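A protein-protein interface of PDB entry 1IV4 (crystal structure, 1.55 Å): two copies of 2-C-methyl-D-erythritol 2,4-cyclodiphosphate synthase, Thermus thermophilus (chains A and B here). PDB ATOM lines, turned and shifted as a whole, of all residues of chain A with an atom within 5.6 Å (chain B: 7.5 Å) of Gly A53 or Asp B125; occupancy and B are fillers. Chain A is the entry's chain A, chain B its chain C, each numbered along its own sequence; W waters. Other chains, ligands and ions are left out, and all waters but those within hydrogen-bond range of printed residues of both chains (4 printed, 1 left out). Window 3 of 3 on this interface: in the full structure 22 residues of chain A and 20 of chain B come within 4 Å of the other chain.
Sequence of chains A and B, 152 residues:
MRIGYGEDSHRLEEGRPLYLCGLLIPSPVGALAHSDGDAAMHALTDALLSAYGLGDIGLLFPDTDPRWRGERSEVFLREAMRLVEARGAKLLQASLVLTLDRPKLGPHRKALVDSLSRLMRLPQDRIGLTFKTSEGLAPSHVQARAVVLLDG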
ATOM      1  N   ARG A   2       5.247 -12.344 -13.942  1.00  0.00           N
ATOM      2  CA  ARG A   2       4.417 -11.205 -13.567  1.00  0.00           C
ATOM      3  C   ARG A   2       4.327 -11.082 -12.051  1.00  0.00           C
ATOM      4  O   ARG A   2       4.419 -12.117 -11.400  1.00  0.00           O
ATOM      5  CB  ARG A   2       2.987 -11.355 -14.083  1.00  0.00           C
ATOM      6  CG  ARG A   2       2.918 -11.133 -15.590  1.00  0.00           C
ATOM      7  CD  ARG A   2       1.475 -11.182 -16.082  1.00  0.00           C
ATOM      8  NE  ARG A   2       1.498 -10.884 -17.511  1.00  0.00           N
ATOM      9  CZ  ARG A   2       1.083  -9.768 -18.071  1.00  0.00           C
ATOM     10  NH1 ARG A   2       0.562  -8.785 -17.364  1.00  0.00           N
ATOM     11  NH2 ARG A   2       1.172  -9.648 -19.390  1.00  0.00           N
ATOM     12  N   LEU A  49      -5.609  -9.514  -9.790  1.00  0.00           N
ATOM     13  CA  LEU A  49      -6.143  -8.659 -10.859  1.00  0.00           C
ATOM     14  C   LEU A  49      -5.095  -7.651 -11.325  1.00  0.00           C
ATOM     15  O   LEU A  49      -4.932  -7.379 -12.520  1.00  0.00           O
ATOM     16  CB  LEU A  49      -7.389  -7.895 -10.399  1.00  0.00           C
ATOM     17  CG  LEU A  49      -8.596  -8.764 -10.019  1.00  0.00           C
ATOM     18  CD1 LEU A  49      -9.704  -7.902  -9.413  1.00  0.00           C
ATOM     19  CD2 LEU A  49      -9.117  -9.531 -11.224  1.00  0.00           C
ATOM     20  N   SER A  50      -4.389  -7.090 -10.355  1.00  0.00           N
ATOM     21  CA  SER A  50      -3.375  -6.089 -10.654  1.00  0.00           C
ATOM     22  C   SER A  50      -2.288  -6.678 -11.562  1.00  0.00           C
ATOM     23  O   SER A  50      -1.775  -5.947 -12.402  1.00  0.00           O
ATOM     24  CB  SER A  50      -2.736  -5.574  -9.362  1.00  0.00           C
ATOM     25  OG  SER A  50      -2.033  -4.371  -9.593  1.00  0.00           O
ATOM     26  N   ALA A  51      -1.958  -7.952 -11.390  1.00  0.00           N
ATOM     27  CA  ALA A  51      -0.879  -8.578 -12.152  1.00  0.00           C
ATOM     28  C   ALA A  51      -1.218  -8.599 -13.640  1.00  0.00           C
ATOM     29  O   ALA A  51      -0.294  -8.794 -14.446  1.00  0.00           O
ATOM     30  CB  ALA A  51      -0.589  -9.981 -11.635  1.00  0.00           C
ATOM     31  N   TYR A  52      -2.481  -8.428 -14.023  1.00  0.00           N
ATOM     32  CA  TYR A  52      -2.848  -8.388 -15.444  1.00  0.00           C
ATOM     33  C   TYR A  52      -3.529  -7.087 -15.812  1.00  0.00           C
ATOM     34  O   TYR A  52      -4.105  -6.906 -16.896  1.00  0.00           O
ATOM     35  CB  TYR A  52      -3.734  -9.613 -15.791  1.00  0.00           C
ATOM     36  CG  TYR A  52      -2.859 -10.782 -16.180  1.00  0.00           C
ATOM     37  CD1 TYR A  52      -2.338 -11.583 -15.176  1.00  0.00           C
ATOM     38  CD2 TYR A  52      -2.540 -11.060 -17.507  1.00  0.00           C
ATOM     39  CE1 TYR A  52      -1.527 -12.657 -15.452  1.00  0.00           C
ATOM     40  CE2 TYR A  52      -1.723 -12.136 -17.784  1.00  0.00           C
ATOM     41  CZ  TYR A  52      -1.229 -12.926 -16.780  1.00  0.00           C
ATOM     42  OH  TYR A  52      -0.404 -14.006 -17.020  1.00  0.00           O
ATOM     43  N   GLY A  53      -3.508  -6.107 -14.912  1.00  0.00           N
ATOM     44  CA  GLY A  53      -4.077  -4.795 -15.197  1.00  0.00           C
ATOM     45  C   GLY A  53      -5.589  -4.826 -15.296  1.00  0.00           C
ATOM     46  O   GLY A  53      -6.186  -3.988 -15.990  1.00  0.00           O
ATOM     47  N   LEU A  54      -6.223  -5.778 -14.607  1.00  0.00           N
ATOM     48  CA  LEU A  54      -7.641  -6.019 -14.882  1.00  0.00           C
ATOM     49  C   LEU A  54      -8.568  -5.141 -14.055  1.00  0.00           C
ATOM     50  O   LEU A  54      -9.782  -5.097 -14.319  1.00  0.00           O
ATOM     51  CB  LEU A  54      -7.999  -7.475 -14.601  1.00  0.00           C
ATOM     52  CG  LEU A  54      -7.267  -8.532 -15.427  1.00  0.00           C
ATOM     53  CD1 LEU A  54      -7.657  -9.938 -15.010  1.00  0.00           C
ATOM     54  CD2 LEU A  54      -7.567  -8.364 -16.911  1.00  0.00           C
ATOM     55  N   GLY A  55      -8.044  -4.450 -13.069  1.00  0.00           N
ATOM     56  CA  GLY A  55      -8.846  -3.519 -12.282  1.00  0.00           C
ATOM     57  C   GLY A  55      -8.715  -3.867 -10.812  1.00  0.00           C
ATOM     58  O   GLY A  55      -7.639  -4.253 -10.363  1.00  0.00           O
ATOM     59  N   LEU B  92       9.506  -3.930 -16.766  1.00  0.00           N
ATOM     60  CA  LEU B  92       8.520  -4.849 -17.295  1.00  0.00           C
ATOM     61  C   LEU B  92       7.130  -4.630 -16.713  1.00  0.00           C
ATOM     62  O   LEU B  92       6.130  -4.918 -17.345  1.00  0.00           O
ATOM     63  CB  LEU B  92       8.981  -6.286 -17.022  1.00  0.00           C
ATOM     64  CG  LEU B  92       8.101  -7.416 -17.558  1.00  0.00           C
ATOM     65  CD1 LEU B  92       8.013  -7.293 -19.066  1.00  0.00           C
ATOM     66  CD2 LEU B  92       8.643  -8.768 -17.125  1.00  0.00           C
ATOM     67  N   GLN B  93       7.038  -4.119 -15.492  1.00  0.00           N
ATOM     68  CA  GLN B  93       5.742  -4.086 -14.811  1.00  0.00           C
ATOM     69  C   GLN B  93       5.757  -3.134 -13.631  1.00  0.00           C
ATOM     70  O   GLN B  93       6.775  -2.980 -12.937  1.00  0.00           O
ATOM     71  CB  GLN B  93       5.320  -5.473 -14.299  1.00  0.00           C
ATOM     72  CG  GLN B  93       3.858  -5.546 -13.846  1.00  0.00           C
ATOM     73  CD  GLN B  93       3.268  -6.935 -13.930  1.00  0.00           C
ATOM     74  OE1 GLN B  93       2.067  -7.085 -14.150  1.00  0.00           O
ATOM     75  NE2 GLN B  93       4.114  -7.926 -13.726  1.00  0.00           N
ATOM     76  N   ALA B  94       4.596  -2.516 -13.389  1.00  0.00           N
ATOM     77  CA  ALA B  94       4.432  -1.691 -12.181  1.00  0.00           C
ATOM     78  C   ALA B  94       3.061  -2.000 -11.580  1.00  0.00           C
ATOM     79  O   ALA B  94       2.048  -2.003 -12.306  1.00  0.00           O
ATOM     80  CB  ALA B  94       4.576  -0.208 -12.446  1.00  0.00           C
ATOM     81  N   ARG B 109     -10.356   5.691 -13.903  1.00  0.00           N
ATOM     82  CA  ARG B 109      -9.470   4.540 -14.079  1.00  0.00           C
ATOM     83  C   ARG B 109      -8.779   4.531 -15.427  1.00  0.00           C
ATOM     84  O   ARG B 109      -7.575   4.330 -15.558  1.00  0.00           O
ATOM     85  CB  ARG B 109     -10.274   3.247 -13.879  1.00  0.00           C
ATOM     86  CG  ARG B 109      -9.416   2.010 -13.698  1.00  0.00           C
ATOM     87  CD  ARG B 109     -10.200   0.757 -13.376  1.00  0.00           C
ATOM     88  NE  ARG B 109     -11.034   0.930 -12.183  1.00  0.00           N
ATOM     89  CZ  ARG B 109     -10.662   0.577 -10.961  1.00  0.00           C
ATOM     90  NH1 ARG B 109      -9.461   0.034 -10.770  1.00  0.00           N
ATOM     91  NH2 ARG B 109     -11.477   0.765  -9.935  1.00  0.00           N
ATOM     92  N   VAL B 113      -4.605   4.876 -15.746  1.00  0.00           N
ATOM     93  CA  VAL B 113      -3.788   3.785 -16.294  1.00  0.00           C
ATOM     94  C   VAL B 113      -3.141   4.217 -17.606  1.00  0.00           C
ATOM     95  O   VAL B 113      -1.966   3.893 -17.846  1.00  0.00           O
ATOM     96  CB  VAL B 113      -4.635   2.515 -16.512  1.00  0.00           C
ATOM     97  CG1 VAL B 113      -3.879   1.428 -17.263  1.00  0.00           C
ATOM     98  CG2 VAL B 113      -5.144   1.975 -15.175  1.00  0.00           C
ATOM     99  N   SER B 117       0.767   4.131 -18.304  1.00  0.00           N
ATOM    100  CA  SER B 117       1.238   3.367 -19.451  1.00  0.00           C
ATOM    101  C   SER B 117       2.128   4.232 -20.321  1.00  0.00           C
ATOM    102  O   SER B 117       3.214   3.835 -20.731  1.00  0.00           O
ATOM    103  CB  SER B 117       0.027   2.817 -20.217  1.00  0.00           C
ATOM    104  OG  SER B 117       0.488   2.253 -21.437  1.00  0.00           O
ATOM    105  N   LEU B 122       4.901   1.226 -20.801  1.00  0.00           N
ATOM    106  CA  LEU B 122       4.460  -0.131 -20.569  1.00  0.00           C
ATOM    107  C   LEU B 122       3.072  -0.381 -21.177  1.00  0.00           C
ATOM    108  O   LEU B 122       2.267   0.547 -21.197  1.00  0.00           O
ATOM    109  CB  LEU B 122       4.375  -0.511 -19.070  1.00  0.00           C
ATOM    110  CG  LEU B 122       5.692  -0.492 -18.307  1.00  0.00           C
ATOM    111  CD1 LEU B 122       5.435  -0.699 -16.815  1.00  0.00           C
ATOM    112  CD2 LEU B 122       6.662  -1.539 -18.825  1.00  0.00           C
ATOM    113  N   PRO B 123       2.867  -1.611 -21.631  1.00  0.00           N
ATOM    114  CA  PRO B 123       1.544  -2.031 -22.136  1.00  0.00           C
ATOM    115  C   PRO B 123       0.519  -1.961 -21.007  1.00  0.00           C
ATOM    116  O   PRO B 123       0.865  -2.075 -19.828  1.00  0.00           O
ATOM    117  CB  PRO B 123       1.729  -3.463 -22.589  1.00  0.00           C
ATOM    118  CG  PRO B 123       3.062  -3.904 -22.118  1.00  0.00           C
ATOM    119  CD  PRO B 123       3.840  -2.708 -21.703  1.00  0.00           C
ATOM    120  N   GLN B 124      -0.751  -1.772 -21.381  1.00  0.00           N
ATOM    121  CA  GLN B 124      -1.732  -1.531 -20.319  1.00  0.00           C
ATOM    122  C   GLN B 124      -1.874  -2.721 -19.377  1.00  0.00           C
ATOM    123  O   GLN B 124      -2.215  -2.532 -18.198  1.00  0.00           O
ATOM    124  CB  GLN B 124      -3.087  -1.135 -20.920  1.00  0.00           C
ATOM    125  CG  GLN B 124      -2.996   0.076 -21.834  1.00  0.00           C
ATOM    126  CD  GLN B 124      -3.853   1.244 -21.392  1.00  0.00           C
ATOM    127  OE1 GLN B 124      -4.773   1.085 -20.584  1.00  0.00           O
ATOM    128  NE2 GLN B 124      -3.569   2.422 -21.941  1.00  0.00           N
ATOM    129  N   ASP B 125      -1.611  -3.936 -19.838  1.00  0.00           N
ATOM    130  CA  ASP B 125      -1.748  -5.105 -18.981  1.00  0.00           C
ATOM    131  C   ASP B 125      -0.603  -5.238 -17.973  1.00  0.00           C
ATOM    132  O   ASP B 125      -0.660  -6.122 -17.115  1.00  0.00           O
ATOM    133  CB  ASP B 125      -1.794  -6.389 -19.833  1.00  0.00           C
ATOM    134  CG  ASP B 125      -0.456  -6.492 -20.567  1.00  0.00           C
ATOM    135  OD1 ASP B 125       0.393  -7.323 -20.200  1.00  0.00           O
ATOM    136  OD2 ASP B 125      -0.259  -5.700 -21.516  1.00  0.00           O
ATOM    137  N   ARG B 126       0.397  -4.384 -18.108  1.00  0.00           N
ATOM    138  CA  ARG B 126       1.585  -4.372 -17.253  1.00  0.00           C
ATOM    139  C   ARG B 126       1.574  -3.178 -16.306  1.00  0.00           C
ATOM    140  O   ARG B 126       2.551  -2.928 -15.587  1.00  0.00           O
ATOM    141  CB  ARG B 126       2.863  -4.373 -18.103  1.00  0.00           C
ATOM    142  CG  ARG B 126       3.170  -5.709 -18.738  1.00  0.00           C
ATOM    143  CD  ARG B 126       3.597  -6.744 -17.702  1.00  0.00           C
ATOM    144  NE  ARG B 126       4.070  -7.966 -18.358  1.00  0.00           N
ATOM    145  CZ  ARG B 126       4.813  -8.897 -17.778  1.00  0.00           C
ATOM    146  NH1 ARG B 126       5.207  -8.800 -16.516  1.00  0.00           N
ATOM    147  NH2 ARG B 126       5.161  -9.952 -18.510  1.00  0.00           N
ATOM    148  N   ILE B 127       0.471  -2.447 -16.266  1.00  0.00           N
ATOM    149  CA  ILE B 127       0.146  -1.413 -15.305  1.00  0.00           C
ATOM    150  C   ILE B 127      -0.941  -1.956 -14.382  1.00  0.00           C
ATOM    151  O   ILE B 127      -2.085  -2.194 -14.812  1.00  0.00           O
ATOM    152  CB  ILE B 127      -0.334  -0.099 -15.948  1.00  0.00           C
ATOM    153  CG1 ILE B 127       0.715   0.531 -16.865  1.00  0.00           C
ATOM    154  CG2 ILE B 127      -0.833   0.888 -14.904  1.00  0.00           C
ATOM    155  CD1 ILE B 127       2.054   0.824 -16.205  1.00  0.00           C
ATOM    156  N   GLY B 128      -0.569  -2.206 -13.140  1.00  0.00           N
ATOM    157  CA  GLY B 128      -1.530  -2.779 -12.193  1.00  0.00           C
ATOM    158  C   GLY B 128      -1.935  -1.757 -11.172  1.00  0.00           C
ATOM    159  O   GLY B 128      -1.217  -1.589 -10.195  1.00  0.00           O
ATOM    160  N   LEU B 129      -3.048  -1.068 -11.388  1.00  0.00           N
ATOM    161  CA  LEU B 129      -3.443   0.025 -10.515  1.00  0.00           C
ATOM    162  C   LEU B 129      -4.733  -0.392  -9.809  1.00  0.00           C
ATOM    163  O   LEU B 129      -5.658  -0.844 -10.479  1.00  0.00           O
ATOM    164  CB  LEU B 129      -3.634   1.293 -11.341  1.00  0.00           C
ATOM    165  CG  LEU B 129      -4.105   2.552 -10.610  1.00  0.00           C
ATOM    166  CD1 LEU B 129      -3.130   3.065  -9.561  1.00  0.00           C
ATOM    167  CD2 LEU B 129      -4.350   3.669 -11.639  1.00  0.00           C
HETATM  168  O   HOH W   1      -2.471  -2.910  -7.357  1.00  0.00           O
HETATM  169  O   HOH W   2      -4.852  -2.534 -17.971  1.00  0.00           O
HETATM  170  O   HOH W   3       3.640  -8.632 -20.910  1.00  0.00           O
HETATM  171  O   HOH W   4      -5.388  -3.680 -12.081  1.00  0.00           O
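The backbone carbonyl oxygen of Ala B94 lies within hydrogen-bond range of the backbone NH of Gly B128, at 2.8 Å. NE2 of Gln B93 lies close to NH1 of Arg B126, 3.1 Å away. The backbone NH of Ala B94 lies within hydrogen-bond range of the backbone carbonyl oxygen of Arg B126 (3.0 Å). The backbone carbonyl oxygen (O) of Ala A51 lies within hydrogen-bond range of the guanidinium group (NH1) of Arg A2 (3.0 Å).
Along chain A the printed residues that touch a printed residue of chain B span positions 2 to 55.
The side-chain hydroxyl (OG) of Ser A50 is in hydrogen-bond range of the backbone carbonyl oxygen (O) of Gly B128 (3.0 Å). OE1 of Gln B93 lies close to O of Ala A51 (2.9 Å). The side-chain carboxylate of Asp B125 is in salt-bridge range of the guanidinium group of Arg A2.
Of the printed residues of chain A, Asp B125 touches Arg A2, Ala A51, Tyr A52 and Gly A53. Of the printed residues of chain B, Ser A50 touches Gly B128 (3.0 Å) and Leu B129 (3.9 Å). Of the printed residues of chain B, Ala A51 touches Gln B93 and Asp B125. Of the printed residues of chain B, Gly A55 touches Arg B109 (3.9 Å) and Leu B129 (3.9 Å). Printed residues of chain A within 4 Å of Ile B127: Gly A53. Printed residues of chain A within 4 Å of Arg B109: Gly A55 (3.9 Å). Ser B117 touches none of the printed residues of chain A. Leu A49 touches none of the printed residues of chain B. The nearest residue of chain A that does not touch Asp B125 is Ser A50 (4.8 Å). The nearest printed residue of chain A that does not touch Arg B126 is Tyr A52 (5.3 Å).
Among the printed residues, pairs that only touch across the chains: Arg A2 with Gln B93 (3.3 Å), Arg A2 with Arg B126 (3.4 Å), Ser A50 with Leu B129 (3.9 Å), Ala A51 with Asp B125 (3.8 Å), Tyr A52 with Asp B125 (3.3 Å), Gly A53 with Asp B125 (3.6 Å), Gly A53 with Ile B127 (3.3 Å), Gly A55 with Arg B109 (3.9 Å) and Gly A55 with Leu B129 (3.9 Å).
Water W2 lies within hydrogen-bond range of the backbone carbonyl oxygen of Gln B124 (2.6 Å) and the backbone carbonyl oxygen of Gly A53 (2.8 Å). Water W3 bridges the guanidinium group (NE) of Arg B126 (2.7 Å) and the guanidinium group (NH2) of Arg A2 (3.1 Å). Water W1 lies within hydrogen-bond range of OG of Ser A50 (2.7 Å) and O of Gly B128 (3.4 Å). Water W4 lies within hydrogen-bond range of the backbone carbonyl oxygen (O) of Gly A55 (2.9 Å), the backbone carbonyl oxygen (O) of Leu B129 (3.3 Å) and the backbone NH (N) of Leu A54 (3.4 Å).
No position is printed for both chains.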
